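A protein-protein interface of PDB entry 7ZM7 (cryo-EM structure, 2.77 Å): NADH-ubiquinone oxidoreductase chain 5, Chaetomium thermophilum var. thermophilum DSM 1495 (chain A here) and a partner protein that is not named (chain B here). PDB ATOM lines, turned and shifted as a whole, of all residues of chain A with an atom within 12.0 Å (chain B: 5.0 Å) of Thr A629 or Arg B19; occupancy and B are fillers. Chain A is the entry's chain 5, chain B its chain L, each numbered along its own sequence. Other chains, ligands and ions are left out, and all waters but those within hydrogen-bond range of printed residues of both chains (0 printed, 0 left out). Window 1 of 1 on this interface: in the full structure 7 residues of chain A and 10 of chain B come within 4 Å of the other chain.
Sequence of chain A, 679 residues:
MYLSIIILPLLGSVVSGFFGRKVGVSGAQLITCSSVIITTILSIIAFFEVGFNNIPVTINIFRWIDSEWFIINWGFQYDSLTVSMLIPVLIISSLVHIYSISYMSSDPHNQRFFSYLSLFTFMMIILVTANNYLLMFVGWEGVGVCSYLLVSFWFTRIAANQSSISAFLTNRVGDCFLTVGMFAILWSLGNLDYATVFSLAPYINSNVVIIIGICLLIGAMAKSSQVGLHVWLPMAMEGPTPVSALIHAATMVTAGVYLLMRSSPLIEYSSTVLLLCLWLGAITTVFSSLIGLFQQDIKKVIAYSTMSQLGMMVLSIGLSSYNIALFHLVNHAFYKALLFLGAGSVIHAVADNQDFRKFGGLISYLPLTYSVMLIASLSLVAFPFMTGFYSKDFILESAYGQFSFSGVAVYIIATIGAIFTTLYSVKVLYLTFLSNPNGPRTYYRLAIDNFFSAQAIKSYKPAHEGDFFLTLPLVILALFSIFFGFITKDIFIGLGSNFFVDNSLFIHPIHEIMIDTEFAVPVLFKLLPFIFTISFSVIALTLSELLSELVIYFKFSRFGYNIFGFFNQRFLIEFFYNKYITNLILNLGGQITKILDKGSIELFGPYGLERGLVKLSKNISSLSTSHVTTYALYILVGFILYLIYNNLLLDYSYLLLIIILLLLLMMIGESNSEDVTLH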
ATOM      1  N   LEU A 623       2.590   9.513 -23.946  1.00  0.00           N
ATOM      2  CA  LEU A 623       3.617   8.514 -23.708  1.00  0.00           C
ATOM      3  C   LEU A 623       3.511   7.333 -24.660  1.00  0.00           C
ATOM      4  O   LEU A 623       4.525   6.705 -24.969  1.00  0.00           O
ATOM      5  CB  LEU A 623       3.526   8.028 -22.264  1.00  0.00           C
ATOM      6  CG  LEU A 623       4.044   9.007 -21.221  1.00  0.00           C
ATOM      7  CD1 LEU A 623       3.474   8.694 -19.855  1.00  0.00           C
ATOM      8  CD2 LEU A 623       5.549   8.946 -21.184  1.00  0.00           C
ATOM      9  N   SER A 624       2.310   7.016 -25.129  1.00  0.00           N
ATOM     10  CA  SER A 624       2.045   5.770 -25.849  1.00  0.00           C
ATOM     11  C   SER A 624       2.367   5.952 -27.324  1.00  0.00           C
ATOM     12  O   SER A 624       1.560   6.480 -28.084  1.00  0.00           O
ATOM     13  CB  SER A 624       0.595   5.351 -25.649  1.00  0.00           C
ATOM     14  OG  SER A 624       0.371   4.953 -24.312  1.00  0.00           O
ATOM     15  N   THR A 625       3.535   5.480 -27.749  1.00  0.00           N
ATOM     16  CA  THR A 625       4.077   5.881 -29.040  1.00  0.00           C
ATOM     17  C   THR A 625       4.202   4.704 -30.009  1.00  0.00           C
ATOM     18  O   THR A 625       4.627   4.885 -31.151  1.00  0.00           O
ATOM     19  CB  THR A 625       5.419   6.573 -28.809  1.00  0.00           C
ATOM     20  OG1 THR A 625       5.202   7.701 -27.961  1.00  0.00           O
ATOM     21  CG2 THR A 625       5.925   7.182 -30.082  1.00  0.00           C
ATOM     22  N   SER A 626       3.784   3.510 -29.591  1.00  0.00           N
ATOM     23  CA  SER A 626       3.912   2.280 -30.370  1.00  0.00           C
ATOM     24  C   SER A 626       5.357   2.016 -30.775  1.00  0.00           C
ATOM     25  O   SER A 626       5.623   1.462 -31.839  1.00  0.00           O
ATOM     26  CB  SER A 626       3.005   2.291 -31.598  1.00  0.00           C
ATOM     27  OG  SER A 626       3.546   3.101 -32.612  1.00  0.00           O
ATOM     28  N   HIS A 627       6.293   2.395 -29.896  1.00  0.00           N
ATOM     29  CA  HIS A 627       7.721   2.078 -30.140  1.00  0.00           C
ATOM     30  C   HIS A 627       8.109   0.961 -29.173  1.00  0.00           C
ATOM     31  O   HIS A 627       8.200   1.240 -27.975  1.00  0.00           O
ATOM     32  CB  HIS A 627       8.607   3.321 -30.009  1.00  0.00           C
ATOM     33  CG  HIS A 627       8.488   4.267 -31.155  1.00  0.00           C
ATOM     34  ND1 HIS A 627       8.773   5.611 -31.034  1.00  0.00           N
ATOM     35  CD2 HIS A 627       8.115   4.072 -32.438  1.00  0.00           C
ATOM     36  CE1 HIS A 627       8.587   6.205 -32.196  1.00  0.00           C
ATOM     37  NE2 HIS A 627       8.181   5.283 -33.073  1.00  0.00           N
ATOM     38  N   VAL A 628       8.269  -0.265 -29.678  1.00  0.00           N
ATOM     39  CA  VAL A 628       8.605  -1.394 -28.824  1.00  0.00           C
ATOM     40  C   VAL A 628       9.834  -1.099 -27.990  1.00  0.00           C
ATOM     41  O   VAL A 628       9.921  -1.518 -26.835  1.00  0.00           O
ATOM     42  CB  VAL A 628       8.755  -2.680 -29.662  1.00  0.00           C
ATOM     43  CG1 VAL A 628       7.457  -3.057 -30.251  1.00  0.00           C
ATOM     44  CG2 VAL A 628       9.657  -2.417 -30.810  1.00  0.00           C
ATOM     45  N   THR A 629      10.789  -0.361 -28.543  1.00  0.00           N
ATOM     46  CA  THR A 629      11.991  -0.044 -27.791  1.00  0.00           C
ATOM     47  C   THR A 629      11.667   0.767 -26.547  1.00  0.00           C
ATOM     48  O   THR A 629      12.210   0.501 -25.471  1.00  0.00           O
ATOM     49  CB  THR A 629      12.980   0.698 -28.685  1.00  0.00           C
ATOM     50  OG1 THR A 629      12.304   1.756 -29.370  1.00  0.00           O
ATOM     51  CG2 THR A 629      13.589  -0.245 -29.695  1.00  0.00           C
ATOM     52  N   THR A 630      10.728   1.712 -26.661  1.00  0.00           N
ATOM     53  CA  THR A 630      10.356   2.582 -25.514  1.00  0.00           C
ATOM     54  C   THR A 630       9.470   1.805 -24.529  1.00  0.00           C
ATOM     55  O   THR A 630       9.571   2.064 -23.318  1.00  0.00           O
ATOM     56  CB  THR A 630       9.786   3.923 -25.987  1.00  0.00           C
ATOM     57  OG1 THR A 630       8.416   3.775 -26.355  1.00  0.00           O
ATOM     58  CG2 THR A 630      10.580   4.527 -27.125  1.00  0.00           C
ATOM     59  N   TYR A 631       8.628   0.907 -25.035  1.00  0.00           N
ATOM     60  CA  TYR A 631       7.743   0.099 -24.160  1.00  0.00           C
ATOM     61  C   TYR A 631       8.572  -0.803 -23.256  1.00  0.00           C
ATOM     62  O   TYR A 631       8.222  -0.948 -22.084  1.00  0.00           O
ATOM     63  CB  TYR A 631       6.710  -0.670 -24.984  1.00  0.00           C
ATOM     64  CG  TYR A 631       5.587   0.174 -25.530  1.00  0.00           C
ATOM     65  CD1 TYR A 631       5.448   1.505 -25.173  1.00  0.00           C
ATOM     66  CD2 TYR A 631       4.655  -0.359 -26.401  1.00  0.00           C
ATOM     67  CE1 TYR A 631       4.421   2.287 -25.674  1.00  0.00           C
ATOM     68  CE2 TYR A 631       3.620   0.404 -26.910  1.00  0.00           C
ATOM     69  CZ  TYR A 631       3.500   1.732 -26.544  1.00  0.00           C
ATOM     70  OH  TYR A 631       2.479   2.485 -27.043  1.00  0.00           O
ATOM     71  N   ALA A 632       9.631  -1.388 -23.792  1.00  0.00           N
ATOM     72  CA  ALA A 632      10.487  -2.308 -23.023  1.00  0.00           C
ATOM     73  C   ALA A 632      11.118  -1.569 -21.847  1.00  0.00           C
ATOM     74  O   ALA A 632      11.158  -2.138 -20.740  1.00  0.00           O
ATOM     75  CB  ALA A 632      11.546  -2.797 -23.953  1.00  0.00           C
ATOM     76  N   LEU A 633      11.584  -0.344 -22.088  1.00  0.00           N
ATOM     77  CA  LEU A 633      12.220   0.464 -21.031  1.00  0.00           C
ATOM     78  C   LEU A 633      11.168   0.738 -19.963  1.00  0.00           C
ATOM     79  O   LEU A 633      11.499   0.615 -18.786  1.00  0.00           O
ATOM     80  CB  LEU A 633      12.739   1.745 -21.687  1.00  0.00           C
ATOM     81  CG  LEU A 633      13.659   2.607 -20.827  1.00  0.00           C
ATOM     82  CD1 LEU A 633      14.797   1.778 -20.257  1.00  0.00           C
ATOM     83  CD2 LEU A 633      14.199   3.779 -21.628  1.00  0.00           C
ATOM     84  N   TYR A 634       9.933   1.033 -20.371  1.00  0.00           N
ATOM     85  CA  TYR A 634       8.859   1.358 -19.399  1.00  0.00           C
ATOM     86  C   TYR A 634       8.577   0.151 -18.501  1.00  0.00           C
ATOM     87  O   TYR A 634       8.356   0.350 -17.298  1.00  0.00           O
ATOM     88  CB  TYR A 634       7.562   1.774 -20.101  1.00  0.00           C
ATOM     89  CG  TYR A 634       7.548   3.083 -20.843  1.00  0.00           C
ATOM     90  CD1 TYR A 634       8.498   4.063 -20.616  1.00  0.00           C
ATOM     91  CD2 TYR A 634       6.552   3.346 -21.769  1.00  0.00           C
ATOM     92  CE1 TYR A 634       8.463   5.266 -21.301  1.00  0.00           C
ATOM     93  CE2 TYR A 634       6.502   4.544 -22.458  1.00  0.00           C
ATOM     94  CZ  TYR A 634       7.464   5.506 -22.225  1.00  0.00           C
ATOM     95  OH  TYR A 634       7.428   6.685 -22.908  1.00  0.00           O
ATOM     96  N   ILE A 635       8.562  -1.051 -19.066  1.00  0.00           N
ATOM     97  CA  ILE A 635       8.321  -2.297 -18.273  1.00  0.00           C
ATOM     98  C   ILE A 635       9.449  -2.501 -17.258  1.00  0.00           C
ATOM     99  O   ILE A 635       9.140  -2.884 -16.124  1.00  0.00           O
ATOM    100  CB  ILE A 635       8.164  -3.517 -19.203  1.00  0.00           C
ATOM    101  CG1 ILE A 635       6.871  -3.447 -20.015  1.00  0.00           C
ATOM    102  CG2 ILE A 635       8.269  -4.825 -18.434  1.00  0.00           C
ATOM    103  CD1 ILE A 635       6.863  -4.359 -21.212  1.00  0.00           C
ATOM    104  N   LEU A 636      10.700  -2.239 -17.651  1.00  0.00           N
ATOM    105  CA  LEU A 636      11.868  -2.391 -16.750  1.00  0.00           C
ATOM    106  C   LEU A 636      11.812  -1.283 -15.708  1.00  0.00           C
ATOM    107  O   LEU A 636      12.118  -1.554 -14.540  1.00  0.00           O
ATOM    108  CB  LEU A 636      13.122  -2.305 -17.617  1.00  0.00           C
ATOM    109  CG  LEU A 636      14.483  -2.277 -16.932  1.00  0.00           C
ATOM    110  CD1 LEU A 636      15.496  -2.946 -17.836  1.00  0.00           C
ATOM    111  CD2 LEU A 636      14.922  -0.846 -16.648  1.00  0.00           C
ATOM    112  N   VAL A 637      11.415  -0.081 -16.119  1.00  0.00           N
ATOM    113  CA  VAL A 637      11.267   0.973 -15.125  1.00  0.00           C
ATOM    114  C   VAL A 637      10.215   0.579 -14.107  1.00  0.00           C
ATOM    115  O   VAL A 637      10.432   0.678 -12.897  1.00  0.00           O
ATOM    116  CB  VAL A 637      10.925   2.311 -15.801  1.00  0.00           C
ATOM    117  CG1 VAL A 637      10.511   3.337 -14.760  1.00  0.00           C
ATOM    118  CG2 VAL A 637      12.110   2.809 -16.591  1.00  0.00           C
ATOM    119  N   GLY A 638       9.071   0.095 -14.584  1.00  0.00           N
ATOM    120  CA  GLY A 638       8.028  -0.360 -13.681  1.00  0.00           C
ATOM    121  C   GLY A 638       8.419  -1.588 -12.890  1.00  0.00           C
ATOM    122  O   GLY A 638       7.849  -1.856 -11.836  1.00  0.00           O
ATOM    123  N   PHE B  15      18.240  -4.005 -23.381  1.00  0.00           N
ATOM    124  CA  PHE B  15      16.962  -3.319 -23.466  1.00  0.00           C
ATOM    125  C   PHE B  15      17.102  -1.862 -23.056  1.00  0.00           C
ATOM    126  O   PHE B  15      16.251  -1.032 -23.386  1.00  0.00           O
ATOM    127  CB  PHE B  15      15.950  -4.032 -22.576  1.00  0.00           C
ATOM    128  CG  PHE B  15      15.187  -5.100 -23.284  1.00  0.00           C
ATOM    129  CD1 PHE B  15      15.673  -6.378 -23.335  1.00  0.00           C
ATOM    130  CD2 PHE B  15      14.008  -4.822 -23.931  1.00  0.00           C
ATOM    131  CE1 PHE B  15      14.979  -7.357 -23.999  1.00  0.00           C
ATOM    132  CE2 PHE B  15      13.311  -5.805 -24.592  1.00  0.00           C
ATOM    133  CZ  PHE B  15      13.794  -7.063 -24.623  1.00  0.00           C
ATOM    134  N   VAL B  16      18.172  -1.547 -22.338  1.00  0.00           N
ATOM    135  CA  VAL B  16      18.397  -0.189 -21.865  1.00  0.00           C
ATOM    136  C   VAL B  16      18.976   0.676 -22.971  1.00  0.00           C
ATOM    137  O   VAL B  16      18.699   1.878 -23.047  1.00  0.00           O
ATOM    138  CB  VAL B  16      19.312  -0.218 -20.634  1.00  0.00           C
ATOM    139  CG1 VAL B  16      19.485   1.166 -20.068  1.00  0.00           C
ATOM    140  CG2 VAL B  16      18.736  -1.158 -19.599  1.00  0.00           C
ATOM    141  N   LEU B  17      19.794   0.091 -23.834  1.00  0.00           N
ATOM    142  CA  LEU B  17      20.531   0.855 -24.822  1.00  0.00           C
ATOM    143  C   LEU B  17      19.923   0.781 -26.210  1.00  0.00           C
ATOM    144  O   LEU B  17      20.572   1.195 -27.175  1.00  0.00           O
ATOM    145  CB  LEU B  17      21.984   0.381 -24.880  1.00  0.00           C
ATOM    146  CG  LEU B  17      22.743   0.440 -23.558  1.00  0.00           C
ATOM    147  CD1 LEU B  17      24.203   0.103 -23.754  1.00  0.00           C
ATOM    148  CD2 LEU B  17      22.591   1.786 -22.929  1.00  0.00           C
ATOM    149  N   ASN B  18      18.709   0.270 -26.348  1.00  0.00           N
ATOM    150  CA  ASN B  18      18.176  -0.042 -27.665  1.00  0.00           C
ATOM    151  C   ASN B  18      16.999   0.865 -27.988  1.00  0.00           C
ATOM    152  O   ASN B  18      15.905   0.690 -27.448  1.00  0.00           O
ATOM    153  CB  ASN B  18      17.773  -1.504 -27.758  1.00  0.00           C
ATOM    154  CG  ASN B  18      17.591  -1.947 -29.176  1.00  0.00           C
ATOM    155  OD1 ASN B  18      17.858  -1.191 -30.101  1.00  0.00           O
ATOM    156  ND2 ASN B  18      17.110  -3.159 -29.364  1.00  0.00           N
ATOM    157  N   ARG B  19      17.216   1.801 -28.908  1.00  0.00           N
ATOM    158  CA  ARG B  19      16.149   2.625 -29.434  1.00  0.00           C
ATOM    159  C   ARG B  19      15.739   2.242 -30.843  1.00  0.00           C
ATOM    160  O   ARG B  19      14.654   2.635 -31.280  1.00  0.00           O
ATOM    161  CB  ARG B  19      16.560   4.102 -29.432  1.00  0.00           C
ATOM    162  CG  ARG B  19      17.017   4.621 -28.099  1.00  0.00           C
ATOM    163  CD  ARG B  19      15.862   5.082 -27.231  1.00  0.00           C
ATOM    164  NE  ARG B  19      15.179   3.967 -26.576  1.00  0.00           N
ATOM    165  CZ  ARG B  19      15.690   3.242 -25.587  1.00  0.00           C
ATOM    166  NH1 ARG B  19      14.986   2.260 -25.061  1.00  0.00           N
ATOM    167  NH2 ARG B  19      16.905   3.498 -25.133  1.00  0.00           N
ATOM    168  N   LYS B  20      16.563   1.489 -31.560  1.00  0.00           N
ATOM    169  CA  LYS B  20      16.317   1.229 -32.966  1.00  0.00           C
ATOM    170  C   LYS B  20      16.372  -0.236 -33.362  1.00  0.00           C
ATOM    171  O   LYS B  20      15.773  -0.587 -34.383  1.00  0.00           O
ATOM    172  CB  LYS B  20      17.323   1.998 -33.822  1.00  0.00           C
ATOM    173  CG  LYS B  20      17.607   3.386 -33.332  1.00  0.00           C
ATOM    174  CD  LYS B  20      16.592   4.349 -33.859  1.00  0.00           C
ATOM    175  CE  LYS B  20      17.176   5.741 -33.913  1.00  0.00           C
ATOM    176  NZ  LYS B  20      18.168   5.850 -35.015  1.00  0.00           N
ATOM    177  N   ASN B  21      17.063  -1.092 -32.610  1.00  0.00           N
ATOM    178  CA  ASN B  21      17.287  -2.486 -32.989  1.00  0.00           C
ATOM    179  C   ASN B  21      16.162  -3.345 -32.447  1.00  0.00           C
ATOM    180  O   ASN B  21      16.191  -3.752 -31.287  1.00  0.00           O
ATOM    181  CB  ASN B  21      18.601  -3.009 -32.423  1.00  0.00           C
ATOM    182  CG  ASN B  21      19.765  -2.715 -33.271  1.00  0.00           C
ATOM    183  OD1 ASN B  21      20.056  -3.447 -34.195  1.00  0.00           O
ATOM    184  ND2 ASN B  21      20.497  -1.680 -32.926  1.00  0.00           N
ATOM    185  N   MET B  25      16.577  -6.535 -29.579  1.00  0.00           N
ATOM    186  CA  MET B  25      15.569  -6.996 -28.629  1.00  0.00           C
ATOM    187  C   MET B  25      15.315  -8.494 -28.765  1.00  0.00           C
ATOM    188  O   MET B  25      15.104  -9.188 -27.771  1.00  0.00           O
ATOM    189  CB  MET B  25      14.270  -6.217 -28.753  1.00  0.00           C
ATOM    190  CG  MET B  25      14.273  -4.945 -27.963  1.00  0.00           C
ATOM    191  SD  MET B  25      12.608  -4.337 -27.746  1.00  0.00           S
ATOM    192  CE  MET B  25      12.145  -4.216 -29.449  1.00  0.00           C
ATOM    193  N   ILE B  86      13.160   1.590 -36.642  1.00  0.00           N
ATOM    194  CA  ILE B  86      12.130   2.341 -35.866  1.00  0.00           C
ATOM    195  C   ILE B  86      12.424   3.826 -36.087  1.00  0.00           C
ATOM    196  O   ILE B  86      13.487   4.286 -35.628  1.00  0.00           O
ATOM    197  CB  ILE B  86      12.196   1.982 -34.369  1.00  0.00           C
ATOM    198  CG1 ILE B  86      11.911   0.502 -34.113  1.00  0.00           C
ATOM    199  CG2 ILE B  86      11.277   2.876 -33.551  1.00  0.00           C
ATOM    200  CD1 ILE B  86      11.500   0.209 -32.693  1.00  0.00           C
ATOM    201  N   TYR B  88      12.648   7.557 -35.285  1.00  0.00           N
ATOM    202  CA  TYR B  88      12.746   8.147 -33.924  1.00  0.00           C
ATOM    203  C   TYR B  88      13.312   9.568 -34.025  1.00  0.00           C
ATOM    204  O   TYR B  88      12.699  10.468 -33.418  1.00  0.00           O
ATOM    205  CB  TYR B  88      13.613   7.255 -33.033  1.00  0.00           C
ATOM    206  CG  TYR B  88      13.378   7.413 -31.552  1.00  0.00           C
ATOM    207  CD1 TYR B  88      12.288   6.819 -30.938  1.00  0.00           C
ATOM    208  CD2 TYR B  88      14.249   8.145 -30.763  1.00  0.00           C
ATOM    209  CE1 TYR B  88      12.065   6.956 -29.578  1.00  0.00           C
ATOM    210  CE2 TYR B  88      14.041   8.290 -29.402  1.00  0.00           C
ATOM    211  CZ  TYR B  88      12.944   7.694 -28.808  1.00  0.00           C
ATOM    212  OH  TYR B  88      12.730   7.834 -27.467  1.00  0.00           O
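O of Arg B19 is in hydrogen-bond range of OG1 of Thr A629, 3.2 Å away.
N of Asn B21 lies within hydrogen-bond range of OD1 of Asn B18 (2.6 Å). The guanidinium group of Arg B19 sits at hydrogen-bond distance from the backbone carbonyl oxygen of Val B16 (3.2 Å). The side-chain hydroxyl (OG1) of Thr A630 sits at hydrogen-bond distance from the backbone carbonyl oxygen (O) of His A627 (3.0 Å). The backbone NH of Lys B20 sits at hydrogen-bond distance from the side-chain amide oxygen of Asn B18 (3.3 Å). The side-chain amide nitrogen (ND2) of Asn B18 lies close to the backbone NH (N) of Met B25 (3.4 Å).
Among the printed residues, pairs that only touch across the chains: Thr A629 with Asn B18 (3.2 Å), Ala A632 with Phe B15 (3.2 Å), Val A628 with Met B25 (3.4 Å), His A627 with Ile B86 (3.6 Å), Thr A629 with Ile B86 (3.7 Å), His A627 with Tyr B88 (3.7 Å), Val A628 with Ile B86 (3.7 Å), Thr A630 with Tyr B88 (3.8 Å), Leu A633 with Arg B19 (3.8 Å) and Thr A629 with Lys B20 (3.9 Å).
Of chain B, only Asn B18, Arg B19, Lys B20 and Ile B86 come within 4 Å of Thr A629. Asn B18 touches just one residue of chain A: Thr A629. No residue of chain A comes within 4 Å of Asn B21. Of chain A, only His A627, Val A628 and Thr A629 come within 4 Å of Ile B86. Of the printed residues of chain B, His A627 touches Ile B86 (3.6 Å) and Tyr B88 (3.7 Å). Of the printed residues of chain A, Met B25 touches Val A628. Printed residues of chain B within 4 Å of Thr A630: Tyr B88 (3.8 Å). Printed residues of chain B within 4 Å of Ala A632: Phe B15 (3.2 Å). The nearest residue of chain A that does not touch Arg B19 is Thr A630 (4.6 Å). The nearest printed residue of chain B that does not touch Leu A633 is Val B16 (4.4 Å).
Of the 16 printed residues of chain A, 6 touch a printed residue of chain B. Hydrophobic or aromatic side chains of chain A within 4 Å of the printed part of chain B: His A627, Val A628, Ala A632 and Leu A633. Along chain A the printed residues that touch a printed residue of chain B span positions 627 to 633. Hydrophobic or aromatic side chains of chain B within 4 Å of the printed part of chain A: Phe B15, Met B25, Ile B86 and Tyr B88. Among the printed residues, 11 pairs touch across the chains.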
